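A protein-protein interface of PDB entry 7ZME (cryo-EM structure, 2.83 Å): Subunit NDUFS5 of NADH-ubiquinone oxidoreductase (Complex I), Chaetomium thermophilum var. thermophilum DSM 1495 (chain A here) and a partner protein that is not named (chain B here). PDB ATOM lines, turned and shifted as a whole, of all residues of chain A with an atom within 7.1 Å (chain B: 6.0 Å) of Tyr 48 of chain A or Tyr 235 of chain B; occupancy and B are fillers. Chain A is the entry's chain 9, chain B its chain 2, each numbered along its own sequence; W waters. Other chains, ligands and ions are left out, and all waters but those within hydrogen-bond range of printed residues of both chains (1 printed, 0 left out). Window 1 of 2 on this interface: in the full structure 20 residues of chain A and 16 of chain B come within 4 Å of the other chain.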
ATOM      1  N   CYS A  14      -3.931  26.325  -7.118  1.00  0.00           N
ATOM      2  CA  CYS A  14      -4.979  25.560  -7.840  1.00  0.00           C
ATOM      3  C   CYS A  14      -4.571  25.347  -9.295  1.00  0.00           C
ATOM      4  O   CYS A  14      -5.460  25.118 -10.103  1.00  0.00           O
ATOM      5  CB  CYS A  14      -6.322  26.276  -7.738  1.00  0.00           C
ATOM      6  SG  CYS A  14      -6.957  26.304  -6.050  1.00  0.00           S
ATOM      7  N   PHE A  17      -4.861  21.403 -10.183  1.00  0.00           N
ATOM      8  CA  PHE A  17      -6.299  21.076 -10.312  1.00  0.00           C
ATOM      9  C   PHE A  17      -6.831  21.562 -11.658  1.00  0.00           C
ATOM     10  O   PHE A  17      -7.718  20.910 -12.218  1.00  0.00           O
ATOM     11  CB  PHE A  17      -7.047  21.623  -9.097  1.00  0.00           C
ATOM     12  CG  PHE A  17      -6.984  20.735  -7.882  1.00  0.00           C
ATOM     13  CD1 PHE A  17      -7.691  19.545  -7.840  1.00  0.00           C
ATOM     14  CD2 PHE A  17      -6.222  21.084  -6.781  1.00  0.00           C
ATOM     15  CE1 PHE A  17      -7.638  18.729  -6.721  1.00  0.00           C
ATOM     16  CE2 PHE A  17      -6.173  20.270  -5.663  1.00  0.00           C
ATOM     17  CZ  PHE A  17      -6.882  19.095  -5.635  1.00  0.00           C
ATOM     18  N   LEU A  21      -7.961  19.228 -15.130  1.00  0.00           N
ATOM     19  CA  LEU A  21      -9.284  19.404 -15.765  1.00  0.00           C
ATOM     20  C   LEU A  21      -9.160  19.638 -17.273  1.00  0.00           C
ATOM     21  O   LEU A  21      -9.932  19.019 -18.025  1.00  0.00           O
ATOM     22  CB  LEU A  21      -9.968  20.581 -15.071  1.00  0.00           C
ATOM     23  CG  LEU A  21     -11.363  20.940 -15.563  1.00  0.00           C
ATOM     24  CD1 LEU A  21     -12.287  19.740 -15.461  1.00  0.00           C
ATOM     25  CD2 LEU A  21     -11.909  22.116 -14.775  1.00  0.00           C
ATOM     26  N   VAL A  43     -13.524  16.084 -11.861  1.00  0.00           N
ATOM     27  CA  VAL A  43     -12.309  16.871 -12.023  1.00  0.00           C
ATOM     28  C   VAL A  43     -12.619  18.359 -11.935  1.00  0.00           C
ATOM     29  O   VAL A  43     -11.822  19.141 -11.406  1.00  0.00           O
ATOM     30  CB  VAL A  43     -11.634  16.502 -13.355  1.00  0.00           C
ATOM     31  CG1 VAL A  43     -10.245  17.049 -13.412  1.00  0.00           C
ATOM     32  CG2 VAL A  43     -11.610  15.001 -13.525  1.00  0.00           C
ATOM     33  N   MET A  44     -13.779  18.774 -12.449  1.00  0.00           N
ATOM     34  CA  MET A  44     -14.150  20.183 -12.403  1.00  0.00           C
ATOM     35  C   MET A  44     -14.614  20.591 -11.013  1.00  0.00           C
ATOM     36  O   MET A  44     -14.451  21.750 -10.621  1.00  0.00           O
ATOM     37  CB  MET A  44     -15.232  20.478 -13.444  1.00  0.00           C
ATOM     38  CG  MET A  44     -15.531  21.963 -13.638  1.00  0.00           C
ATOM     39  SD  MET A  44     -17.005  22.296 -14.612  1.00  0.00           S
ATOM     40  CE  MET A  44     -18.184  21.217 -13.812  1.00  0.00           C
ATOM     41  N   GLU A  45     -15.193  19.656 -10.261  1.00  0.00           N
ATOM     42  CA  GLU A  45     -15.573  19.935  -8.881  1.00  0.00           C
ATOM     43  C   GLU A  45     -14.352  20.090  -7.985  1.00  0.00           C
ATOM     44  O   GLU A  45     -14.374  20.889  -7.043  1.00  0.00           O
ATOM     45  CB  GLU A  45     -16.481  18.821  -8.365  1.00  0.00           C
ATOM     46  CG  GLU A  45     -17.011  19.035  -6.966  1.00  0.00           C
ATOM     47  CD  GLU A  45     -17.942  17.925  -6.525  1.00  0.00           C
ATOM     48  OE1 GLU A  45     -18.149  16.977  -7.316  1.00  0.00           O
ATOM     49  OE2 GLU A  45     -18.472  17.999  -5.397  1.00  0.00           O
ATOM     50  N   ASP A  46     -13.285  19.340  -8.257  1.00  0.00           N
ATOM     51  CA  ASP A  46     -12.068  19.465  -7.465  1.00  0.00           C
ATOM     52  C   ASP A  46     -11.408  20.817  -7.677  1.00  0.00           C
ATOM     53  O   ASP A  46     -10.814  21.377  -6.750  1.00  0.00           O
ATOM     54  CB  ASP A  46     -11.093  18.344  -7.816  1.00  0.00           C
ATOM     55  CG  ASP A  46     -11.602  16.987  -7.418  1.00  0.00           C
ATOM     56  OD1 ASP A  46     -12.471  16.921  -6.531  1.00  0.00           O
ATOM     57  OD2 ASP A  46     -11.134  15.988  -7.992  1.00  0.00           O
ATOM     58  N   TYR A  47     -11.474  21.342  -8.902  1.00  0.00           N
ATOM     59  CA  TYR A  47     -10.899  22.652  -9.176  1.00  0.00           C
ATOM     60  C   TYR A  47     -11.642  23.745  -8.422  1.00  0.00           C
ATOM     61  O   TYR A  47     -11.021  24.656  -7.866  1.00  0.00           O
ATOM     62  CB  TYR A  47     -10.909  22.926 -10.680  1.00  0.00           C
ATOM     63  CG  TYR A  47     -10.590  24.359 -11.031  1.00  0.00           C
ATOM     64  CD1 TYR A  47      -9.310  24.863 -10.875  1.00  0.00           C
ATOM     65  CD2 TYR A  47     -11.577  25.212 -11.496  1.00  0.00           C
ATOM     66  CE1 TYR A  47      -9.019  26.170 -11.183  1.00  0.00           C
ATOM     67  CE2 TYR A  47     -11.296  26.517 -11.804  1.00  0.00           C
ATOM     68  CZ  TYR A  47     -10.016  26.993 -11.647  1.00  0.00           C
ATOM     69  OH  TYR A  47      -9.736  28.301 -11.961  1.00  0.00           O
ATOM     70  N   TYR A  48     -12.974  23.675  -8.394  1.00  0.00           N
ATOM     71  CA  TYR A  48     -13.743  24.641  -7.619  1.00  0.00           C
ATOM     72  C   TYR A  48     -13.509  24.456  -6.125  1.00  0.00           C
ATOM     73  O   TYR A  48     -13.519  25.430  -5.365  1.00  0.00           O
ATOM     74  CB  TYR A  48     -15.231  24.518  -7.943  1.00  0.00           C
ATOM     75  CG  TYR A  48     -15.656  25.134  -9.257  1.00  0.00           C
ATOM     76  CD1 TYR A  48     -15.423  26.474  -9.533  1.00  0.00           C
ATOM     77  CD2 TYR A  48     -16.305  24.377 -10.217  1.00  0.00           C
ATOM     78  CE1 TYR A  48     -15.817  27.034 -10.733  1.00  0.00           C
ATOM     79  CE2 TYR A  48     -16.703  24.927 -11.414  1.00  0.00           C
ATOM     80  CZ  TYR A  48     -16.462  26.252 -11.668  1.00  0.00           C
ATOM     81  OH  TYR A  48     -16.863  26.788 -12.865  1.00  0.00           O
ATOM     82  N   GLU A  49     -13.318  23.213  -5.683  1.00  0.00           N
ATOM     83  CA  GLU A  49     -13.075  22.961  -4.268  1.00  0.00           C
ATOM     84  C   GLU A  49     -11.723  23.506  -3.834  1.00  0.00           C
ATOM     85  O   GLU A  49     -11.610  24.117  -2.766  1.00  0.00           O
ATOM     86  CB  GLU A  49     -13.179  21.465  -3.979  1.00  0.00           C
ATOM     87  CG  GLU A  49     -13.119  21.067  -2.509  1.00  0.00           C
ATOM     88  CD  GLU A  49     -13.832  22.026  -1.568  1.00  0.00           C
ATOM     89  OE1 GLU A  49     -14.931  22.514  -1.901  1.00  0.00           O
ATOM     90  OE2 GLU A  49     -13.287  22.287  -0.479  1.00  0.00           O
ATOM     91  N   CYS A  50     -10.686  23.298  -4.650  1.00  0.00           N
ATOM     92  CA  CYS A  50      -9.398  23.938  -4.404  1.00  0.00           C
ATOM     93  C   CYS A  50      -9.543  25.445  -4.320  1.00  0.00           C
ATOM     94  O   CYS A  50      -8.820  26.106  -3.570  1.00  0.00           O
ATOM     95  CB  CYS A  50      -8.411  23.574  -5.516  1.00  0.00           C
ATOM     96  SG  CYS A  50      -6.765  24.360  -5.453  1.00  0.00           S
ATOM     97  N   LEU A  51     -10.459  26.040  -5.065  1.00  0.00           N
ATOM     98  CA  LEU A  51     -10.586  27.519  -5.142  1.00  0.00           C
ATOM     99  C   LEU A  51     -11.385  28.118  -3.977  1.00  0.00           C
ATOM    100  O   LEU A  51     -10.879  29.070  -3.374  1.00  0.00           O
ATOM    101  CB  LEU A  51     -11.298  27.791  -6.468  1.00  0.00           C
ATOM    102  CG  LEU A  51     -10.726  28.863  -7.390  1.00  0.00           C
ATOM    103  CD1 LEU A  51      -9.313  28.519  -7.818  1.00  0.00           C
ATOM    104  CD2 LEU A  51     -11.614  29.012  -8.612  1.00  0.00           C
ATOM    105  N   HIS A  52     -12.587  27.610  -3.690  1.00  0.00           N
ATOM    106  CA  HIS A  52     -13.485  28.235  -2.688  1.00  0.00           C
ATOM    107  C   HIS A  52     -13.527  27.512  -1.332  1.00  0.00           C
ATOM    108  O   HIS A  52     -13.890  28.190  -0.356  1.00  0.00           O
ATOM    109  CB  HIS A  52     -14.838  28.428  -3.375  1.00  0.00           C
ATOM    110  CG  HIS A  52     -14.690  29.101  -4.698  1.00  0.00           C
ATOM    111  ND1 HIS A  52     -14.086  30.337  -4.828  1.00  0.00           N
ATOM    112  CD2 HIS A  52     -15.029  28.712  -5.944  1.00  0.00           C
ATOM    113  CE1 HIS A  52     -14.070  30.683  -6.095  1.00  0.00           C
ATOM    114  NE2 HIS A  52     -14.646  29.707  -6.798  1.00  0.00           N
ATOM    115  N   HIS A  53     -13.207  26.214  -1.265  1.00  0.00           N
ATOM    116  CA  HIS A  53     -13.128  25.464   0.022  1.00  0.00           C
ATOM    117  C   HIS A  53     -14.482  25.299   0.730  1.00  0.00           C
ATOM    118  O   HIS A  53     -14.456  25.145   1.952  1.00  0.00           O
ATOM    119  CB  HIS A  53     -12.119  26.099   0.989  1.00  0.00           C
ATOM    120  CG  HIS A  53     -10.822  26.513   0.385  1.00  0.00           C
ATOM    121  ND1 HIS A  53      -9.855  25.605   0.018  1.00  0.00           N
ATOM    122  CD2 HIS A  53     -10.316  27.735   0.121  1.00  0.00           C
ATOM    123  CE1 HIS A  53      -8.815  26.248  -0.464  1.00  0.00           C
ATOM    124  NE2 HIS A  53      -9.074  27.554  -0.413  1.00  0.00           N
ATOM    125  N   ARG A  54     -15.604  25.295   0.007  1.00  0.00           N
ATOM    126  CA  ARG A  54     -16.950  25.098   0.612  1.00  0.00           C
ATOM    127  C   ARG A  54     -17.130  23.688   1.172  1.00  0.00           C
ATOM    128  O   ARG A  54     -17.739  23.570   2.241  1.00  0.00           O
ATOM    129  CB  ARG A  54     -18.073  25.422  -0.371  1.00  0.00           C
ATOM    130  CG  ARG A  54     -17.900  26.741  -1.110  1.00  0.00           C
ATOM    131  CD  ARG A  54     -19.146  27.162  -1.867  1.00  0.00           C
ATOM    132  NE  ARG A  54     -20.119  27.835  -1.020  1.00  0.00           N
ATOM    133  CZ  ARG A  54     -21.196  27.263  -0.492  1.00  0.00           C
ATOM    134  NH1 ARG A  54     -22.013  27.973   0.265  1.00  0.00           N
ATOM    135  NH2 ARG A  54     -21.458  25.991  -0.729  1.00  0.00           N
ATOM    136  N   LYS A  55     -16.641  22.663   0.469  1.00  0.00           N
ATOM    137  CA  LYS A  55     -16.828  21.262   0.922  1.00  0.00           C
ATOM    138  C   LYS A  55     -15.923  20.998   2.124  1.00  0.00           C
ATOM    139  O   LYS A  55     -16.316  20.197   2.973  1.00  0.00           O
ATOM    140  CB  LYS A  55     -16.583  20.256  -0.208  1.00  0.00           C
ATOM    141  CG  LYS A  55     -17.362  20.483  -1.492  1.00  0.00           C
ATOM    142  CD  LYS A  55     -16.957  19.529  -2.584  1.00  0.00           C
ATOM    143  CE  LYS A  55     -17.177  18.084  -2.192  1.00  0.00           C
ATOM    144  NZ  LYS A  55     -16.621  17.149  -3.199  1.00  0.00           N
ATOM    145  N   GLU A  56     -14.754  21.632   2.183  1.00  0.00           N
ATOM    146  CA  GLU A  56     -13.809  21.351   3.293  1.00  0.00           C
ATOM    147  C   GLU A  56     -14.242  22.157   4.506  1.00  0.00           C
ATOM    148  O   GLU A  56     -13.970  21.729   5.639  1.00  0.00           O
ATOM    149  CB  GLU A  56     -12.387  21.772   2.938  1.00  0.00           C
ATOM    150  CG  GLU A  56     -11.358  21.427   3.996  1.00  0.00           C
ATOM    151  CD  GLU A  56     -10.083  22.253   3.951  1.00  0.00           C
ATOM    152  OE1 GLU A  56      -9.836  22.907   2.919  1.00  0.00           O
ATOM    153  OE2 GLU A  56      -9.344  22.244   4.951  1.00  0.00           O
ATOM    154  N   ASN B 200     -15.006  34.024  -9.654  1.00  0.00           N
ATOM    155  CA  ASN B 200     -15.711  32.774  -9.414  1.00  0.00           C
ATOM    156  C   ASN B 200     -15.093  31.589 -10.137  1.00  0.00           C
ATOM    157  O   ASN B 200     -15.244  30.452  -9.683  1.00  0.00           O
ATOM    158  CB  ASN B 200     -17.174  32.917  -9.826  1.00  0.00           C
ATOM    159  CG  ASN B 200     -18.064  33.333  -8.681  1.00  0.00           C
ATOM    160  OD1 ASN B 200     -18.494  32.501  -7.890  1.00  0.00           O
ATOM    161  ND2 ASN B 200     -18.351  34.622  -8.588  1.00  0.00           N
ATOM    162  N   SER B 201     -14.399  31.824 -11.246  1.00  0.00           N
ATOM    163  CA  SER B 201     -13.808  30.754 -12.034  1.00  0.00           C
ATOM    164  C   SER B 201     -12.301  30.640 -11.866  1.00  0.00           C
ATOM    165  O   SER B 201     -11.717  29.664 -12.346  1.00  0.00           O
ATOM    166  CB  SER B 201     -14.132  30.952 -13.515  1.00  0.00           C
ATOM    167  OG  SER B 201     -13.796  32.262 -13.928  1.00  0.00           O
ATOM    168  N   LEU B 212     -15.342  25.379 -18.834  1.00  0.00           N
ATOM    169  CA  LEU B 212     -16.125  25.232 -17.576  1.00  0.00           C
ATOM    170  C   LEU B 212     -17.627  25.222 -17.896  1.00  0.00           C
ATOM    171  O   LEU B 212     -18.334  24.413 -17.296  1.00  0.00           O
ATOM    172  CB  LEU B 212     -15.754  26.356 -16.605  1.00  0.00           C
ATOM    173  CG  LEU B 212     -14.330  26.331 -16.056  1.00  0.00           C
ATOM    174  CD1 LEU B 212     -13.984  27.658 -15.405  1.00  0.00           C
ATOM    175  CD2 LEU B 212     -14.146  25.193 -15.069  1.00  0.00           C
ATOM    176  N   SER B 233     -23.018  19.232  -7.168  1.00  0.00           N
ATOM    177  CA  SER B 233     -24.055  19.508  -6.182  1.00  0.00           C
ATOM    178  C   SER B 233     -23.628  20.621  -5.233  1.00  0.00           C
ATOM    179  O   SER B 233     -24.448  21.178  -4.505  1.00  0.00           O
ATOM    180  CB  SER B 233     -24.394  18.243  -5.391  1.00  0.00           C
ATOM    181  OG  SER B 233     -25.143  17.332  -6.177  1.00  0.00           O
ATOM    182  N   TRP B 234     -22.331  20.942  -5.246  1.00  0.00           N
ATOM    183  CA  TRP B 234     -21.787  21.981  -4.384  1.00  0.00           C
ATOM    184  C   TRP B 234     -21.388  23.247  -5.124  1.00  0.00           C
ATOM    185  O   TRP B 234     -21.364  24.316  -4.510  1.00  0.00           O
ATOM    186  CB  TRP B 234     -20.566  21.456  -3.617  1.00  0.00           C
ATOM    187  CG  TRP B 234     -20.931  20.552  -2.489  1.00  0.00           C
ATOM    188  CD1 TRP B 234     -21.400  19.276  -2.581  1.00  0.00           C
ATOM    189  CD2 TRP B 234     -20.882  20.863  -1.093  1.00  0.00           C
ATOM    190  NE1 TRP B 234     -21.634  18.767  -1.327  1.00  0.00           N
ATOM    191  CE2 TRP B 234     -21.325  19.724  -0.397  1.00  0.00           C
ATOM    192  CE3 TRP B 234     -20.500  21.992  -0.365  1.00  0.00           C
ATOM    193  CZ2 TRP B 234     -21.396  19.681   0.990  1.00  0.00           C
ATOM    194  CZ3 TRP B 234     -20.572  21.949   1.007  1.00  0.00           C
ATOM    195  CH2 TRP B 234     -21.018  20.803   1.671  1.00  0.00           C
ATOM    196  N   TYR B 235     -21.075  23.156  -6.413  1.00  0.00           N
ATOM    197  CA  TYR B 235     -20.649  24.304  -7.208  1.00  0.00           C
ATOM    198  C   TYR B 235     -21.499  24.331  -8.474  1.00  0.00           C
ATOM    199  O   TYR B 235     -21.095  23.812  -9.515  1.00  0.00           O
ATOM    200  CB  TYR B 235     -19.157  24.220  -7.525  1.00  0.00           C
ATOM    201  CG  TYR B 235     -18.272  24.295  -6.305  1.00  0.00           C
ATOM    202  CD1 TYR B 235     -17.942  25.518  -5.738  1.00  0.00           C
ATOM    203  CD2 TYR B 235     -17.774  23.141  -5.712  1.00  0.00           C
ATOM    204  CE1 TYR B 235     -17.135  25.589  -4.620  1.00  0.00           C
ATOM    205  CE2 TYR B 235     -16.970  23.203  -4.597  1.00  0.00           C
ATOM    206  CZ  TYR B 235     -16.654  24.428  -4.054  1.00  0.00           C
ATOM    207  OH  TYR B 235     -15.854  24.493  -2.942  1.00  0.00           O
ATOM    208  N   LYS B 236     -22.674  24.937  -8.380  1.00  0.00           N
ATOM    209  CA  LYS B 236     -23.389  25.074  -9.640  1.00  0.00           C
ATOM    210  C   LYS B 236     -22.940  26.346 -10.349  1.00  0.00           C
ATOM    211  O   LYS B 236     -22.774  27.388  -9.708  1.00  0.00           O
ATOM    212  CB  LYS B 236     -24.897  25.111  -9.410  1.00  0.00           C
ATOM    213  CG  LYS B 236     -25.485  23.773  -8.988  1.00  0.00           C
ATOM    214  CD  LYS B 236     -27.005  23.782  -9.063  1.00  0.00           C
ATOM    215  CE  LYS B 236     -27.623  24.280  -7.767  1.00  0.00           C
ATOM    216  NZ  LYS B 236     -27.508  23.280  -6.671  1.00  0.00           N
ATOM    217  N   PRO B 237     -22.740  26.298 -11.656  1.00  0.00           N
ATOM    218  CA  PRO B 237     -22.142  27.420 -12.388  1.00  0.00           C
ATOM    219  C   PRO B 237     -23.136  28.536 -12.688  1.00  0.00           C
ATOM    220  O   PRO B 237     -23.269  28.988 -13.827  1.00  0.00           O
ATOM    221  CB  PRO B 237     -21.636  26.752 -13.670  1.00  0.00           C
ATOM    222  CG  PRO B 237     -22.565  25.602 -13.876  1.00  0.00           C
ATOM    223  CD  PRO B 237     -23.222  25.250 -12.570  1.00  0.00           C
ATOM    224  N   TYR B 239     -22.917  31.604 -11.688  1.00  0.00           N
ATOM    225  CA  TYR B 239     -22.255  32.889 -11.869  1.00  0.00           C
ATOM    226  C   TYR B 239     -22.035  33.222 -13.335  1.00  0.00           C
ATOM    227  O   TYR B 239     -22.014  34.401 -13.696  1.00  0.00           O
ATOM    228  CB  TYR B 239     -20.920  32.897 -11.125  1.00  0.00           C
ATOM    229  CG  TYR B 239     -19.887  31.956 -11.700  1.00  0.00           C
ATOM    230  CD1 TYR B 239     -19.848  30.624 -11.324  1.00  0.00           C
ATOM    231  CD2 TYR B 239     -18.945  32.402 -12.618  1.00  0.00           C
ATOM    232  CE1 TYR B 239     -18.908  29.768 -11.842  1.00  0.00           C
ATOM    233  CE2 TYR B 239     -17.998  31.552 -13.140  1.00  0.00           C
ATOM    234  CZ  TYR B 239     -17.986  30.236 -12.749  1.00  0.00           C
ATOM    235  OH  TYR B 239     -17.050  29.377 -13.268  1.00  0.00           O
HETATM  236  O   HOH W   1     -17.752  29.078  -7.804  1.00  0.00           O
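O of Asn 200 of chain B is in hydrogen-bond range of NE2 of His 52 of chain A. The backbone carbonyl oxygen (O) of Ser 201 of chain B lies within hydrogen-bond range of the side-chain hydroxyl (OH) of Tyr 47 of chain A (2.4 Å). The backbone carbonyl oxygen of Tyr 48 of chain A lies within hydrogen-bond range of the side-chain hydroxyl of Tyr 235 of chain B, 3.5 Å away. The side-chain carboxylate of Glu 49 of chain A sits at hydrogen-bond distance from the side-chain hydroxyl of Tyr 235 of chain B (2.4 Å). N of Arg 54 of chain A lies within hydrogen-bond range of OH of Tyr 235 of chain B (3.1 Å). OH of Tyr 239 of chain B lies within hydrogen-bond range of OH of Tyr 48 of chain A, at 2.6 Å. The backbone carbonyl oxygen of Leu 212 of chain B lies close to the side-chain sulfur of Met 44 of chain A, 3.7 Å away.
NZ of Lys 55 of chain A is in salt-bridge range of OE2 of Glu 45 of chain A (3.0 Å). The backbone NH (N) of Arg 54 of chain A sits at hydrogen-bond distance from the side-chain carboxylate (OE1) of Glu 49 of chain A (3.4 Å). The side-chain carboxylate of Glu 49 of chain A sits at hydrogen-bond distance from the backbone NH of Lys 55 of chain A (2.9 Å). The backbone NH (N) of Glu 56 of chain A lies within hydrogen-bond range of the side-chain carboxylate (OE2) of Glu 49 of chain A. A ring nitrogen (NE2) of His 53 of chain A lies close to the backbone carbonyl oxygen of Cys 50 of chain A. The side-chain sulfur of Cys 50 of chain A forms a disulfide with the side-chain sulfur of Cys 14 of chain A.
Leu 21 of chain A touches Leu 212 of chain B (CD2 to CD2, 3.8 Å). O of Asn 200 of chain B touches CE1 of Tyr 48 of chain A, at 3.6 Å. Leu 212 of chain B touches Tyr 48 of chain A. CD2 of Leu 51 of chain A touches C of Ser 201 of chain B (3.7 Å). CE1 of Tyr 235 of chain B touches CB of His 52 of chain A, 3.9 Å away. Tyr 235 of chain B touches His 53 of chain A (OH to N, 3.6 Å). O of Arg 54 of chain A touches CZ3 of Trp 234 of chain B (3.5 Å). CD2 of Trp 234 of chain B touches CG of Lys 55 of chain A, 3.6 Å away. Lys 55 of chain A touches Tyr 235 of chain B (N to OH, 3.95 Å).
Tyr 48 of chain A touches just these residues of chain B: Asn 200 (3.6 Å), Leu 212 (3.8 Å), Tyr 235 (3.5 Å) and Tyr 239 (2.6 Å). Tyr 235 of chain B touches just these residues of chain A: Tyr 48, Glu 49, His 52, His 53, Arg 54 and Lys 55. Printed residues of chain B within 4 Å of Tyr 47 of chain A: Ser 201 (2.4 Å). Printed residues of chain A within 4 Å of Trp 234 of chain B: Arg 54 and Lys 55. Printed residues of chain B within 4 Å of Lys 55 of chain A: Trp 234 (3.6 Å) and Tyr 235 (3.95 Å). Printed residues of chain B within 4 Å of Met 44 of chain A: Leu 212. Printed residues of chain A within 4 Å of Leu 212 of chain B: Leu 21, Met 44 and Tyr 48. The nearest residue of chain B that does not touch Tyr 48 of chain A is Ser 201 of chain B (4.4 Å).
Along chain A the printed residues that touch a printed residue of chain B span positions 21 to 55. Among the printed residues, 16 pairs touch across the chains. Among the printed residues, no Asp or Glu carboxylate lies within 4 Å of a Lys or Arg side-chain nitrogen of the other chain.
Water W1 lies within hydrogen-bond range of a ring nitrogen (NE2) of His 52 of chain A (3.3 Å) and the backbone carbonyl oxygen of Asn 200 of chain B (3.4 Å).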
